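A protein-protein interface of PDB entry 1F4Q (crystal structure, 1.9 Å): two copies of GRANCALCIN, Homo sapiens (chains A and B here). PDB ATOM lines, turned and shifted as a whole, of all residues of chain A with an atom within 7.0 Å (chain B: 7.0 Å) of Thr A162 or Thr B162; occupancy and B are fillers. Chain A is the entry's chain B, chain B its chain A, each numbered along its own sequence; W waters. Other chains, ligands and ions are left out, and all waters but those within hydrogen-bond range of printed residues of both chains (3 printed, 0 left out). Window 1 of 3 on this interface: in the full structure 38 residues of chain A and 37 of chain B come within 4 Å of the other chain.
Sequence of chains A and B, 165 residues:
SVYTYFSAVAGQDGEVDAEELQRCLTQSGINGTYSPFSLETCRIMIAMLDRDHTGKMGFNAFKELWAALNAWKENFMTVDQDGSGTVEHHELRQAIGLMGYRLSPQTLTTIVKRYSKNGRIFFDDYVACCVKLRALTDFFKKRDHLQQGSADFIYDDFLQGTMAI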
ATOM      1  N   ARG A 114      -6.652  33.694  -0.406  1.00  0.00           N
ATOM      2  CA  ARG A 114      -7.656  34.355   0.422  1.00  0.00           C
ATOM      3  C   ARG A 114      -7.049  35.244   1.506  1.00  0.00           C
ATOM      4  O   ARG A 114      -7.623  36.271   1.862  1.00  0.00           O
ATOM      5  CB  ARG A 114      -8.563  33.327   1.108  1.00  0.00           C
ATOM      6  CG  ARG A 114      -9.619  33.984   1.997  1.00  0.00           C
ATOM      7  CD  ARG A 114     -10.456  32.966   2.731  1.00  0.00           C
ATOM      8  NE  ARG A 114     -11.709  33.536   3.218  1.00  0.00           N
ATOM      9  CZ  ARG A 114     -11.828  34.343   4.270  1.00  0.00           C
ATOM     10  NH1 ARG A 114     -10.764  34.691   4.978  1.00  0.00           N
ATOM     11  NH2 ARG A 114     -13.023  34.788   4.622  1.00  0.00           N
ATOM     12  N   LYS A 132      -9.730  27.358  11.575  1.00  0.00           N
ATOM     13  CA  LYS A 132     -10.776  27.060  10.611  1.00  0.00           C
ATOM     14  C   LYS A 132     -10.582  25.689   9.969  1.00  0.00           C
ATOM     15  O   LYS A 132     -11.552  24.977   9.728  1.00  0.00           O
ATOM     16  CB  LYS A 132     -10.833  28.149   9.539  1.00  0.00           C
ATOM     17  CG  LYS A 132     -12.148  28.153   8.771  1.00  0.00           C
ATOM     18  CD  LYS A 132     -12.228  29.350   7.828  1.00  0.00           C
ATOM     19  CE  LYS A 132     -13.601  29.460   7.192  1.00  0.00           C
ATOM     20  NZ  LYS A 132     -13.672  30.666   6.305  1.00  0.00           N
ATOM     21  N   LEU A 136     -13.516  22.889  10.462  1.00  0.00           N
ATOM     22  CA  LEU A 136     -14.185  22.362   9.275  1.00  0.00           C
ATOM     23  C   LEU A 136     -13.934  20.867   9.120  1.00  0.00           C
ATOM     24  O   LEU A 136     -14.814  20.126   8.664  1.00  0.00           O
ATOM     25  CB  LEU A 136     -13.714  23.099   8.013  1.00  0.00           C
ATOM     26  CG  LEU A 136     -14.158  24.561   7.890  1.00  0.00           C
ATOM     27  CD1 LEU A 136     -13.372  25.242   6.781  1.00  0.00           C
ATOM     28  CD2 LEU A 136     -15.659  24.623   7.603  1.00  0.00           C
ATOM     29  N   PHE A 139     -16.045  19.047  11.736  1.00  0.00           N
ATOM     30  CA  PHE A 139     -17.420  19.081  11.263  1.00  0.00           C
ATOM     31  C   PHE A 139     -17.620  18.039  10.156  1.00  0.00           C
ATOM     32  O   PHE A 139     -18.576  17.262  10.184  1.00  0.00           O
ATOM     33  CB  PHE A 139     -17.730  20.490  10.737  1.00  0.00           C
ATOM     34  CG  PHE A 139     -19.066  20.625  10.065  1.00  0.00           C
ATOM     35  CD1 PHE A 139     -20.246  20.577  10.801  1.00  0.00           C
ATOM     36  CD2 PHE A 139     -19.141  20.836   8.689  1.00  0.00           C
ATOM     37  CE1 PHE A 139     -21.486  20.745  10.178  1.00  0.00           C
ATOM     38  CE2 PHE A 139     -20.373  21.005   8.054  1.00  0.00           C
ATOM     39  CZ  PHE A 139     -21.550  20.961   8.800  1.00  0.00           C
ATOM     40  N   PHE A 153     -24.277  15.795   2.804  1.00  0.00           N
ATOM     41  CA  PHE A 153     -24.925  16.739   3.713  1.00  0.00           C
ATOM     42  C   PHE A 153     -26.327  17.171   3.327  1.00  0.00           C
ATOM     43  O   PHE A 153     -26.626  17.386   2.153  1.00  0.00           O
ATOM     44  CB  PHE A 153     -24.109  18.033   3.840  1.00  0.00           C
ATOM     45  CG  PHE A 153     -22.734  17.855   4.398  1.00  0.00           C
ATOM     46  CD1 PHE A 153     -21.687  17.446   3.582  1.00  0.00           C
ATOM     47  CD2 PHE A 153     -22.470  18.153   5.731  1.00  0.00           C
ATOM     48  CE1 PHE A 153     -20.398  17.343   4.081  1.00  0.00           C
ATOM     49  CE2 PHE A 153     -21.183  18.055   6.242  1.00  0.00           C
ATOM     50  CZ  PHE A 153     -20.142  17.650   5.415  1.00  0.00           C
ATOM     51  N   TYR A 155     -28.887  20.099   3.288  1.00  0.00           N
ATOM     52  CA  TYR A 155     -28.703  21.552   3.256  1.00  0.00           C
ATOM     53  C   TYR A 155     -28.719  22.304   4.588  1.00  0.00           C
ATOM     54  O   TYR A 155     -27.797  23.073   4.872  1.00  0.00           O
ATOM     55  CB  TYR A 155     -29.718  22.189   2.312  1.00  0.00           C
ATOM     56  CG  TYR A 155     -29.619  23.700   2.230  1.00  0.00           C
ATOM     57  CD1 TYR A 155     -30.572  24.512   2.844  1.00  0.00           C
ATOM     58  CD2 TYR A 155     -28.592  24.317   1.516  1.00  0.00           C
ATOM     59  CE1 TYR A 155     -30.513  25.906   2.741  1.00  0.00           C
ATOM     60  CE2 TYR A 155     -28.522  25.714   1.408  1.00  0.00           C
ATOM     61  CZ  TYR A 155     -29.490  26.499   2.021  1.00  0.00           C
ATOM     62  OH  TYR A 155     -29.463  27.875   1.890  1.00  0.00           O
ATOM     63  N   ASP A 157     -28.228  21.218   7.585  1.00  0.00           N
ATOM     64  CA  ASP A 157     -27.129  20.780   8.449  1.00  0.00           C
ATOM     65  C   ASP A 157     -25.827  21.390   7.937  1.00  0.00           C
ATOM     66  O   ASP A 157     -24.964  21.816   8.715  1.00  0.00           O
ATOM     67  CB  ASP A 157     -27.025  19.249   8.448  1.00  0.00           C
ATOM     68  CG  ASP A 157     -25.924  18.734   9.360  1.00  0.00           C
ATOM     69  OD1 ASP A 157     -25.859  19.178  10.527  1.00  0.00           O
ATOM     70  OD2 ASP A 157     -25.132  17.870   8.921  1.00  0.00           O
ATOM     71  N   PHE A 158     -25.693  21.419   6.617  1.00  0.00           N
ATOM     72  CA  PHE A 158     -24.517  21.999   5.986  1.00  0.00           C
ATOM     73  C   PHE A 158     -24.420  23.489   6.325  1.00  0.00           C
ATOM     74  O   PHE A 158     -23.368  23.964   6.764  1.00  0.00           O
ATOM     75  CB  PHE A 158     -24.599  21.832   4.474  1.00  0.00           C
ATOM     76  CG  PHE A 158     -23.521  22.560   3.731  1.00  0.00           C
ATOM     77  CD1 PHE A 158     -22.257  22.001   3.590  1.00  0.00           C
ATOM     78  CD2 PHE A 158     -23.763  23.819   3.192  1.00  0.00           C
ATOM     79  CE1 PHE A 158     -21.252  22.681   2.921  1.00  0.00           C
ATOM     80  CE2 PHE A 158     -22.753  24.508   2.518  1.00  0.00           C
ATOM     81  CZ  PHE A 158     -21.504  23.938   2.386  1.00  0.00           C
ATOM     82  N   LEU A 159     -25.516  24.220   6.117  1.00  0.00           N
ATOM     83  CA  LEU A 159     -25.543  25.656   6.391  1.00  0.00           C
ATOM     84  C   LEU A 159     -25.316  25.997   7.856  1.00  0.00           C
ATOM     85  O   LEU A 159     -24.645  26.980   8.162  1.00  0.00           O
ATOM     86  CB  LEU A 159     -26.866  26.283   5.944  1.00  0.00           C
ATOM     87  CG  LEU A 159     -26.881  27.149   4.677  1.00  0.00           C
ATOM     88  CD1 LEU A 159     -28.174  27.958   4.655  1.00  0.00           C
ATOM     89  CD2 LEU A 159     -25.690  28.093   4.647  1.00  0.00           C
ATOM     90  N   GLN A 160     -25.881  25.203   8.760  1.00  0.00           N
ATOM     91  CA  GLN A 160     -25.703  25.468  10.182  1.00  0.00           C
ATOM     92  C   GLN A 160     -24.230  25.410  10.550  1.00  0.00           C
ATOM     93  O   GLN A 160     -23.692  26.345  11.145  1.00  0.00           O
ATOM     94  CB  GLN A 160     -26.465  24.449  11.042  1.00  0.00           C
ATOM     95  CG  GLN A 160     -26.117  24.560  12.531  1.00  0.00           C
ATOM     96  CD  GLN A 160     -26.943  23.647  13.420  1.00  0.00           C
ATOM     97  OE1 GLN A 160     -26.882  22.421  13.305  1.00  0.00           O
ATOM     98  NE2 GLN A 160     -27.721  24.245  14.316  1.00  0.00           N
ATOM     99  N   GLY A 161     -23.585  24.306  10.187  1.00  0.00           N
ATOM    100  CA  GLY A 161     -22.182  24.120  10.511  1.00  0.00           C
ATOM    101  C   GLY A 161     -21.215  25.099   9.871  1.00  0.00           C
ATOM    102  O   GLY A 161     -20.321  25.633  10.543  1.00  0.00           O
ATOM    103  N   THR A 162     -21.382  25.344   8.576  1.00  0.00           N
ATOM    104  CA  THR A 162     -20.484  26.253   7.874  1.00  0.00           C
ATOM    105  C   THR A 162     -20.746  27.724   8.191  1.00  0.00           C
ATOM    106  O   THR A 162     -19.836  28.541   8.099  1.00  0.00           O
ATOM    107  CB  THR A 162     -20.522  26.002   6.353  1.00  0.00           C
ATOM    108  OG1 THR A 162     -21.861  26.136   5.868  1.00  0.00           O
ATOM    109  CG2 THR A 162     -20.015  24.592   6.050  1.00  0.00           C
ATOM    110  N   MET A 163     -21.973  28.067   8.584  1.00  0.00           N
ATOM    111  CA  MET A 163     -22.259  29.455   8.957  1.00  0.00           C
ATOM    112  C   MET A 163     -21.687  29.706  10.357  1.00  0.00           C
ATOM    113  O   MET A 163     -21.201  30.801  10.671  1.00  0.00           O
ATOM    114  CB  MET A 163     -23.766  29.730   8.949  1.00  0.00           C
ATOM    115  CG  MET A 163     -24.360  29.989   7.567  1.00  0.00           C
ATOM    116  SD  MET A 163     -23.683  31.469   6.762  1.00  0.00           S
ATOM    117  CE  MET A 163     -24.381  32.760   7.793  1.00  0.00           C
ATOM    118  N   ALA A 164     -21.726  28.677  11.193  1.00  0.00           N
ATOM    119  CA  ALA A 164     -21.207  28.789  12.548  1.00  0.00           C
ATOM    120  C   ALA A 164     -19.697  29.009  12.559  1.00  0.00           C
ATOM    121  O   ALA A 164     -19.189  29.831  13.324  1.00  0.00           O
ATOM    122  CB  ALA A 164     -21.550  27.535  13.335  1.00  0.00           C
ATOM    123  N   ILE A 165     -18.989  28.277  11.701  1.00  0.00           N
ATOM    124  CA  ILE A 165     -17.531  28.350  11.618  1.00  0.00           C
ATOM    125  C   ILE A 165     -17.051  29.546  10.806  1.00  0.00           C
ATOM    126  O   ILE A 165     -16.278  30.353  11.361  1.00  0.00           O
ATOM    127  CB  ILE A 165     -16.955  27.052  11.002  1.00  0.00           C
ATOM    128  CG1 ILE A 165     -17.292  25.864  11.909  1.00  0.00           C
ATOM    129  CG2 ILE A 165     -15.436  27.172  10.810  1.00  0.00           C
ATOM    130  CD1 ILE A 165     -17.046  24.490  11.266  1.00  0.00           C
ATOM    131  OXT ILE A 165     -17.444  29.658   9.627  1.00  0.00           O
ATOM    132  N   ARG B 114     -23.748  33.553  16.513  1.00  0.00           N
ATOM    133  CA  ARG B 114     -22.363  33.781  16.096  1.00  0.00           C
ATOM    134  C   ARG B 114     -22.030  35.262  16.055  1.00  0.00           C
ATOM    135  O   ARG B 114     -20.912  35.664  16.383  1.00  0.00           O
ATOM    136  CB  ARG B 114     -22.074  33.190  14.713  1.00  0.00           C
ATOM    137  CG  ARG B 114     -20.606  33.353  14.263  1.00  0.00           C
ATOM    138  CD  ARG B 114     -20.375  32.787  12.860  1.00  0.00           C
ATOM    139  NE  ARG B 114     -18.973  32.466  12.584  1.00  0.00           N
ATOM    140  CZ  ARG B 114     -18.048  33.350  12.217  1.00  0.00           C
ATOM    141  NH1 ARG B 114     -18.361  34.631  12.075  1.00  0.00           N
ATOM    142  NH2 ARG B 114     -16.797  32.964  12.010  1.00  0.00           N
ATOM    143  N   LYS B 132     -22.365  35.583   3.215  1.00  0.00           N
ATOM    144  CA  LYS B 132     -21.944  34.217   3.502  1.00  0.00           C
ATOM    145  C   LYS B 132     -23.053  33.203   3.229  1.00  0.00           C
ATOM    146  O   LYS B 132     -22.792  32.101   2.739  1.00  0.00           O
ATOM    147  CB  LYS B 132     -21.467  34.114   4.954  1.00  0.00           C
ATOM    148  CG  LYS B 132     -20.636  32.866   5.243  1.00  0.00           C
ATOM    149  CD  LYS B 132     -20.078  32.882   6.672  1.00  0.00           C
ATOM    150  CE  LYS B 132     -19.219  31.653   6.945  1.00  0.00           C
ATOM    151  NZ  LYS B 132     -18.705  31.624   8.345  1.00  0.00           N
ATOM    152  N   LEU B 136     -22.285  30.328   0.511  1.00  0.00           N
ATOM    153  CA  LEU B 136     -22.401  28.928   0.909  1.00  0.00           C
ATOM    154  C   LEU B 136     -23.510  28.183   0.163  1.00  0.00           C
ATOM    155  O   LEU B 136     -23.326  27.036  -0.242  1.00  0.00           O
ATOM    156  CB  LEU B 136     -22.636  28.817   2.421  1.00  0.00           C
ATOM    157  CG  LEU B 136     -21.434  29.133   3.318  1.00  0.00           C
ATOM    158  CD1 LEU B 136     -21.875  29.180   4.777  1.00  0.00           C
ATOM    159  CD2 LEU B 136     -20.356  28.079   3.115  1.00  0.00           C
ATOM    160  N   PHE B 139     -22.433  27.477  -3.441  1.00  0.00           N
ATOM    161  CA  PHE B 139     -21.459  26.392  -3.398  1.00  0.00           C
ATOM    162  C   PHE B 139     -22.157  25.047  -3.216  1.00  0.00           C
ATOM    163  O   PHE B 139     -21.851  24.076  -3.909  1.00  0.00           O
ATOM    164  CB  PHE B 139     -20.484  26.640  -2.238  1.00  0.00           C
ATOM    165  CG  PHE B 139     -19.475  25.542  -2.032  1.00  0.00           C
ATOM    166  CD1 PHE B 139     -18.569  25.209  -3.035  1.00  0.00           C
ATOM    167  CD2 PHE B 139     -19.411  24.863  -0.820  1.00  0.00           C
ATOM    168  CE1 PHE B 139     -17.609  24.217  -2.831  1.00  0.00           C
ATOM    169  CE2 PHE B 139     -18.456  23.870  -0.603  1.00  0.00           C
ATOM    170  CZ  PHE B 139     -17.550  23.547  -1.613  1.00  0.00           C
ATOM    171  N   PHE B 153     -19.808  15.668  -0.785  1.00  0.00           N
ATOM    172  CA  PHE B 153     -18.586  16.452  -0.848  1.00  0.00           C
ATOM    173  C   PHE B 153     -17.413  15.531  -0.591  1.00  0.00           C
ATOM    174  O   PHE B 153     -17.448  14.714   0.325  1.00  0.00           O
ATOM    175  CB  PHE B 153     -18.552  17.564   0.205  1.00  0.00           C
ATOM    176  CG  PHE B 153     -19.480  18.702  -0.081  1.00  0.00           C
ATOM    177  CD1 PHE B 153     -20.768  18.715   0.447  1.00  0.00           C
ATOM    178  CD2 PHE B 153     -19.069  19.766  -0.881  1.00  0.00           C
ATOM    179  CE1 PHE B 153     -21.634  19.776   0.182  1.00  0.00           C
ATOM    180  CE2 PHE B 153     -19.922  20.826  -1.151  1.00  0.00           C
ATOM    181  CZ  PHE B 153     -21.210  20.835  -0.619  1.00  0.00           C
ATOM    182  N   TYR B 155     -13.799  15.355   0.757  1.00  0.00           N
ATOM    183  CA  TYR B 155     -13.083  16.221   1.709  1.00  0.00           C
ATOM    184  C   TYR B 155     -12.332  17.420   1.130  1.00  0.00           C
ATOM    185  O   TYR B 155     -12.580  18.560   1.520  1.00  0.00           O
ATOM    186  CB  TYR B 155     -12.113  15.386   2.544  1.00  0.00           C
ATOM    187  CG  TYR B 155     -11.301  16.186   3.542  1.00  0.00           C
ATOM    188  CD1 TYR B 155      -9.909  16.213   3.466  1.00  0.00           C
ATOM    189  CD2 TYR B 155     -11.921  16.899   4.572  1.00  0.00           C
ATOM    190  CE1 TYR B 155      -9.146  16.926   4.389  1.00  0.00           C
ATOM    191  CE2 TYR B 155     -11.163  17.624   5.509  1.00  0.00           C
ATOM    192  CZ  TYR B 155      -9.778  17.628   5.407  1.00  0.00           C
ATOM    193  OH  TYR B 155      -9.014  18.331   6.314  1.00  0.00           O
ATOM    194  N   ASP B 157     -12.565  18.937  -1.731  1.00  0.00           N
ATOM    195  CA  ASP B 157     -13.449  19.900  -2.400  1.00  0.00           C
ATOM    196  C   ASP B 157     -14.215  20.719  -1.360  1.00  0.00           C
ATOM    197  O   ASP B 157     -14.416  21.933  -1.510  1.00  0.00           O
ATOM    198  CB  ASP B 157     -14.437  19.165  -3.321  1.00  0.00           C
ATOM    199  CG  ASP B 157     -15.415  20.108  -4.006  1.00  0.00           C
ATOM    200  OD1 ASP B 157     -14.970  21.138  -4.552  1.00  0.00           O
ATOM    201  OD2 ASP B 157     -16.630  19.822  -4.012  1.00  0.00           O
ATOM    202  N   PHE B 158     -14.640  20.039  -0.302  1.00  0.00           N
ATOM    203  CA  PHE B 158     -15.373  20.673   0.787  1.00  0.00           C
ATOM    204  C   PHE B 158     -14.503  21.747   1.429  1.00  0.00           C
ATOM    205  O   PHE B 158     -14.951  22.874   1.636  1.00  0.00           O
ATOM    206  CB  PHE B 158     -15.764  19.628   1.839  1.00  0.00           C
ATOM    207  CG  PHE B 158     -16.393  20.212   3.075  1.00  0.00           C
ATOM    208  CD1 PHE B 158     -17.742  20.559   3.092  1.00  0.00           C
ATOM    209  CD2 PHE B 158     -15.630  20.433   4.217  1.00  0.00           C
ATOM    210  CE1 PHE B 158     -18.323  21.114   4.229  1.00  0.00           C
ATOM    211  CE2 PHE B 158     -16.203  20.989   5.362  1.00  0.00           C
ATOM    212  CZ  PHE B 158     -17.549  21.331   5.367  1.00  0.00           C
ATOM    213  N   LEU B 159     -13.260  21.389   1.746  1.00  0.00           N
ATOM    214  CA  LEU B 159     -12.332  22.329   2.358  1.00  0.00           C
ATOM    215  C   LEU B 159     -12.010  23.509   1.456  1.00  0.00           C
ATOM    216  O   LEU B 159     -11.938  24.644   1.920  1.00  0.00           O
ATOM    217  CB  LEU B 159     -11.021  21.643   2.747  1.00  0.00           C
ATOM    218  CG  LEU B 159     -10.901  20.984   4.118  1.00  0.00           C
ATOM    219  CD1 LEU B 159      -9.417  20.765   4.406  1.00  0.00           C
ATOM    220  CD2 LEU B 159     -11.516  21.868   5.202  1.00  0.00           C
ATOM    221  N   GLN B 160     -11.802  23.254   0.169  1.00  0.00           N
ATOM    222  CA  GLN B 160     -11.484  24.348  -0.742  1.00  0.00           C
ATOM    223  C   GLN B 160     -12.586  25.397  -0.775  1.00  0.00           C
ATOM    224  O   GLN B 160     -12.312  26.601  -0.703  1.00  0.00           O
ATOM    225  CB  GLN B 160     -11.245  23.836  -2.163  1.00  0.00           C
ATOM    226  CG  GLN B 160     -11.111  24.968  -3.176  1.00  0.00           C
ATOM    227  CD  GLN B 160     -10.645  24.493  -4.538  1.00  0.00           C
ATOM    228  OE1 GLN B 160     -11.266  23.626  -5.155  1.00  0.00           O
ATOM    229  NE2 GLN B 160      -9.548  25.067  -5.019  1.00  0.00           N
ATOM    230  N   GLY B 161     -13.832  24.945  -0.882  1.00  0.00           N
ATOM    231  CA  GLY B 161     -14.943  25.878  -0.934  1.00  0.00           C
ATOM    232  C   GLY B 161     -15.189  26.618   0.370  1.00  0.00           C
ATOM    233  O   GLY B 161     -15.377  27.841   0.380  1.00  0.00           O
ATOM    234  N   THR B 162     -15.189  25.884   1.477  1.00  0.00           N
ATOM    235  CA  THR B 162     -15.435  26.495   2.779  1.00  0.00           C
ATOM    236  C   THR B 162     -14.282  27.346   3.320  1.00  0.00           C
ATOM    237  O   THR B 162     -14.513  28.240   4.134  1.00  0.00           O
ATOM    238  CB  THR B 162     -15.827  25.431   3.826  1.00  0.00           C
ATOM    239  OG1 THR B 162     -14.832  24.407   3.864  1.00  0.00           O
ATOM    240  CG2 THR B 162     -17.173  24.806   3.462  1.00  0.00           C
ATOM    241  N   MET B 163     -13.049  27.078   2.889  1.00  0.00           N
ATOM    242  CA  MET B 163     -11.923  27.894   3.346  1.00  0.00           C
ATOM    243  C   MET B 163     -11.883  29.183   2.520  1.00  0.00           C
ATOM    244  O   MET B 163     -11.420  30.221   2.990  1.00  0.00           O
ATOM    245  CB  MET B 163     -10.593  27.148   3.196  1.00  0.00           C
ATOM    246  CG  MET B 163     -10.325  26.071   4.247  1.00  0.00           C
ATOM    247  SD  MET B 163     -10.210  26.716   5.942  1.00  0.00           S
ATOM    248  CE  MET B 163      -8.728  27.777   5.812  1.00  0.00           C
ATOM    249  N   ALA B 164     -12.377  29.115   1.287  1.00  0.00           N
ATOM    250  CA  ALA B 164     -12.398  30.287   0.416  1.00  0.00           C
ATOM    251  C   ALA B 164     -13.453  31.273   0.902  1.00  0.00           C
ATOM    252  O   ALA B 164     -13.202  32.472   0.987  1.00  0.00           O
ATOM    253  CB  ALA B 164     -12.692  29.874  -1.029  1.00  0.00           C
ATOM    254  N   ILE B 165     -14.631  30.758   1.233  1.00  0.00           N
ATOM    255  CA  ILE B 165     -15.728  31.590   1.708  1.00  0.00           C
ATOM    256  C   ILE B 165     -15.511  32.038   3.152  1.00  0.00           C
ATOM    257  O   ILE B 165     -15.800  33.215   3.441  1.00  0.00           O
ATOM    258  CB  ILE B 165     -17.072  30.842   1.610  1.00  0.00           C
ATOM    259  CG1 ILE B 165     -17.349  30.473   0.149  1.00  0.00           C
ATOM    260  CG2 ILE B 165     -18.198  31.717   2.151  1.00  0.00           C
ATOM    261  CD1 ILE B 165     -18.564  29.571  -0.049  1.00  0.00           C
ATOM    262  OXT ILE B 165     -15.071  31.207   3.975  1.00  0.00           O
HETATM  263  O   HOH W   1     -15.177  31.866   9.244  1.00  0.00           O
HETATM  264  O   HOH W   2     -15.929  33.184   6.251  1.00  0.00           O
HETATM  265  O   HOH W   3     -16.629  29.285   5.118  1.00  0.00           O
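Of chain B, only Lys B132, Leu B136 and Thr B162 come within 4 Å of Thr A162. No residue of chain B comes within 4 Å of Gly A161. No residue of chain A comes within 4 Å of Gly B161. Of the printed residues of chain B, Phe A153 touches Phe B153. Of the printed residues of chain B, Phe A158 touches Leu B136 (3.8 Å), Phe B139 (3.9 Å), Phe B153 (3.99 Å) and Phe B158 (3.6 Å). Printed residues of chain B within 4 Å of Leu A159: Leu B136 (3.8 Å). Gln B160 touches none of the printed residues of chain A. The nearest residue of chain A that does not touch Thr B162 is Phe A158 (4.5 Å). The nearest printed residue of chain A that does not touch Leu B136 is Tyr A155 (5.6 Å).
The guanidinium group (NE) of Arg B114 lies close to the backbone carbonyl oxygen (O) of Met A163 (3.4 Å). The guanidinium group (NE) of Arg B114 lies within hydrogen-bond range of the backbone carbonyl oxygen (O) of Ala A164. The guanidinium group (NH2) of Arg B114 lies within salt-bridge range of the chain-end carboxylate (O) of Ile A165 (2.7 Å). The side-chain amino group of Lys B132 lies within hydrogen-bond range of the backbone carbonyl oxygen of Thr A162, at 3.3 Å. The chain-end carboxylate of Ile A165 is in salt-bridge range of the side-chain amino group of Lys B132 (2.7 Å). NZ of Lys A132 is in hydrogen-bond range of O of Thr B162. NE of Arg A114 lies close to O of Met B163, at 3.3 Å. The backbone carbonyl oxygen of Ala B164 is in hydrogen-bond range of the guanidinium group of Arg A114, at 2.9 Å. O of Ile B165 lies within salt-bridge range of NH2 of Arg A114 (3.4 Å). The chain-end carboxylate of Ile B165 is in salt-bridge range of the side-chain amino group of Lys A132 (2.8 Å).
Water W3 lies within hydrogen-bond range of the backbone carbonyl oxygen (O) of Thr B162 (2.6 Å), the chain-end carboxylate (OXT) of Ile B165 (2.7 Å) and the side-chain amino group (NZ) of Lys A132 (3.5 Å). Water W2 bridges O of Ile B165 (2.8 Å) and NZ of Lys A132 (3.4 Å). Water W1 bridges the chain-end carboxylate of Ile A165 (2.8 Å) and the guanidinium group of Arg B114 (3.4 Å).
Of the 15 printed residues of chain B, 11 touch a printed residue of chain A. Printed residues of chain B that touch a printed residue of chain A: Arg B114, Lys B132, Leu B136, Phe B139, Phe B153, Phe B158, Leu B159, Thr B162, Met B163, Ala B164 and Ile B165. Hydrophobic or aromatic side chains of chain B that line the printed part of chain A: Leu B136, Phe B139, Phe B153, Phe B158, Leu B159 and Met B163.
Arg A114 touches Ile B165, and with the chains exchanged Ile A165 touches Arg B114. Lys A132 touches Thr B162, and with the chains exchanged Thr A162 touches Lys B132. Leu A136 touches Leu B159, and with the chains exchanged Leu A159 touches Leu B136. Phe A158 touches Phe B153, but with the chains exchanged Phe A153 does not touch Phe B158 (4.1 Å). 15 positions are printed for both chains.
Met B163 touches Lys A132. CE2 of Phe B158 touches O of Leu A136, at 3.7 Å. Leu A136 touches Thr B162. Phe B158 touches Phe A139 (CZ to CD2, 3.7 Å). CE2 of Phe A158 touches O of Leu B136 (3.8 Å). Phe B153 touches Phe A158 (CZ to CE1, 3.99 Å). CD2 of Leu A159 touches CB of Leu B136, at 3.8 Å. Thr A162 touches Leu B136. Thr B162 touches Thr A162. Met A163 touches Leu B136 (SD to CD1, 3.5 Å).
OG1 of Thr B162 is in hydrogen-bond range of O of Phe B158 (2.7 Å). The side-chain hydroxyl (OG1) of Thr B162 sits at hydrogen-bond distance from the backbone carbonyl oxygen (O) of Leu B159 (3.5 Å). The backbone carbonyl oxygen (O) of Phe A158 is in hydrogen-bond range of the side-chain hydroxyl (OG1) of Thr A162 (2.8 Å).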
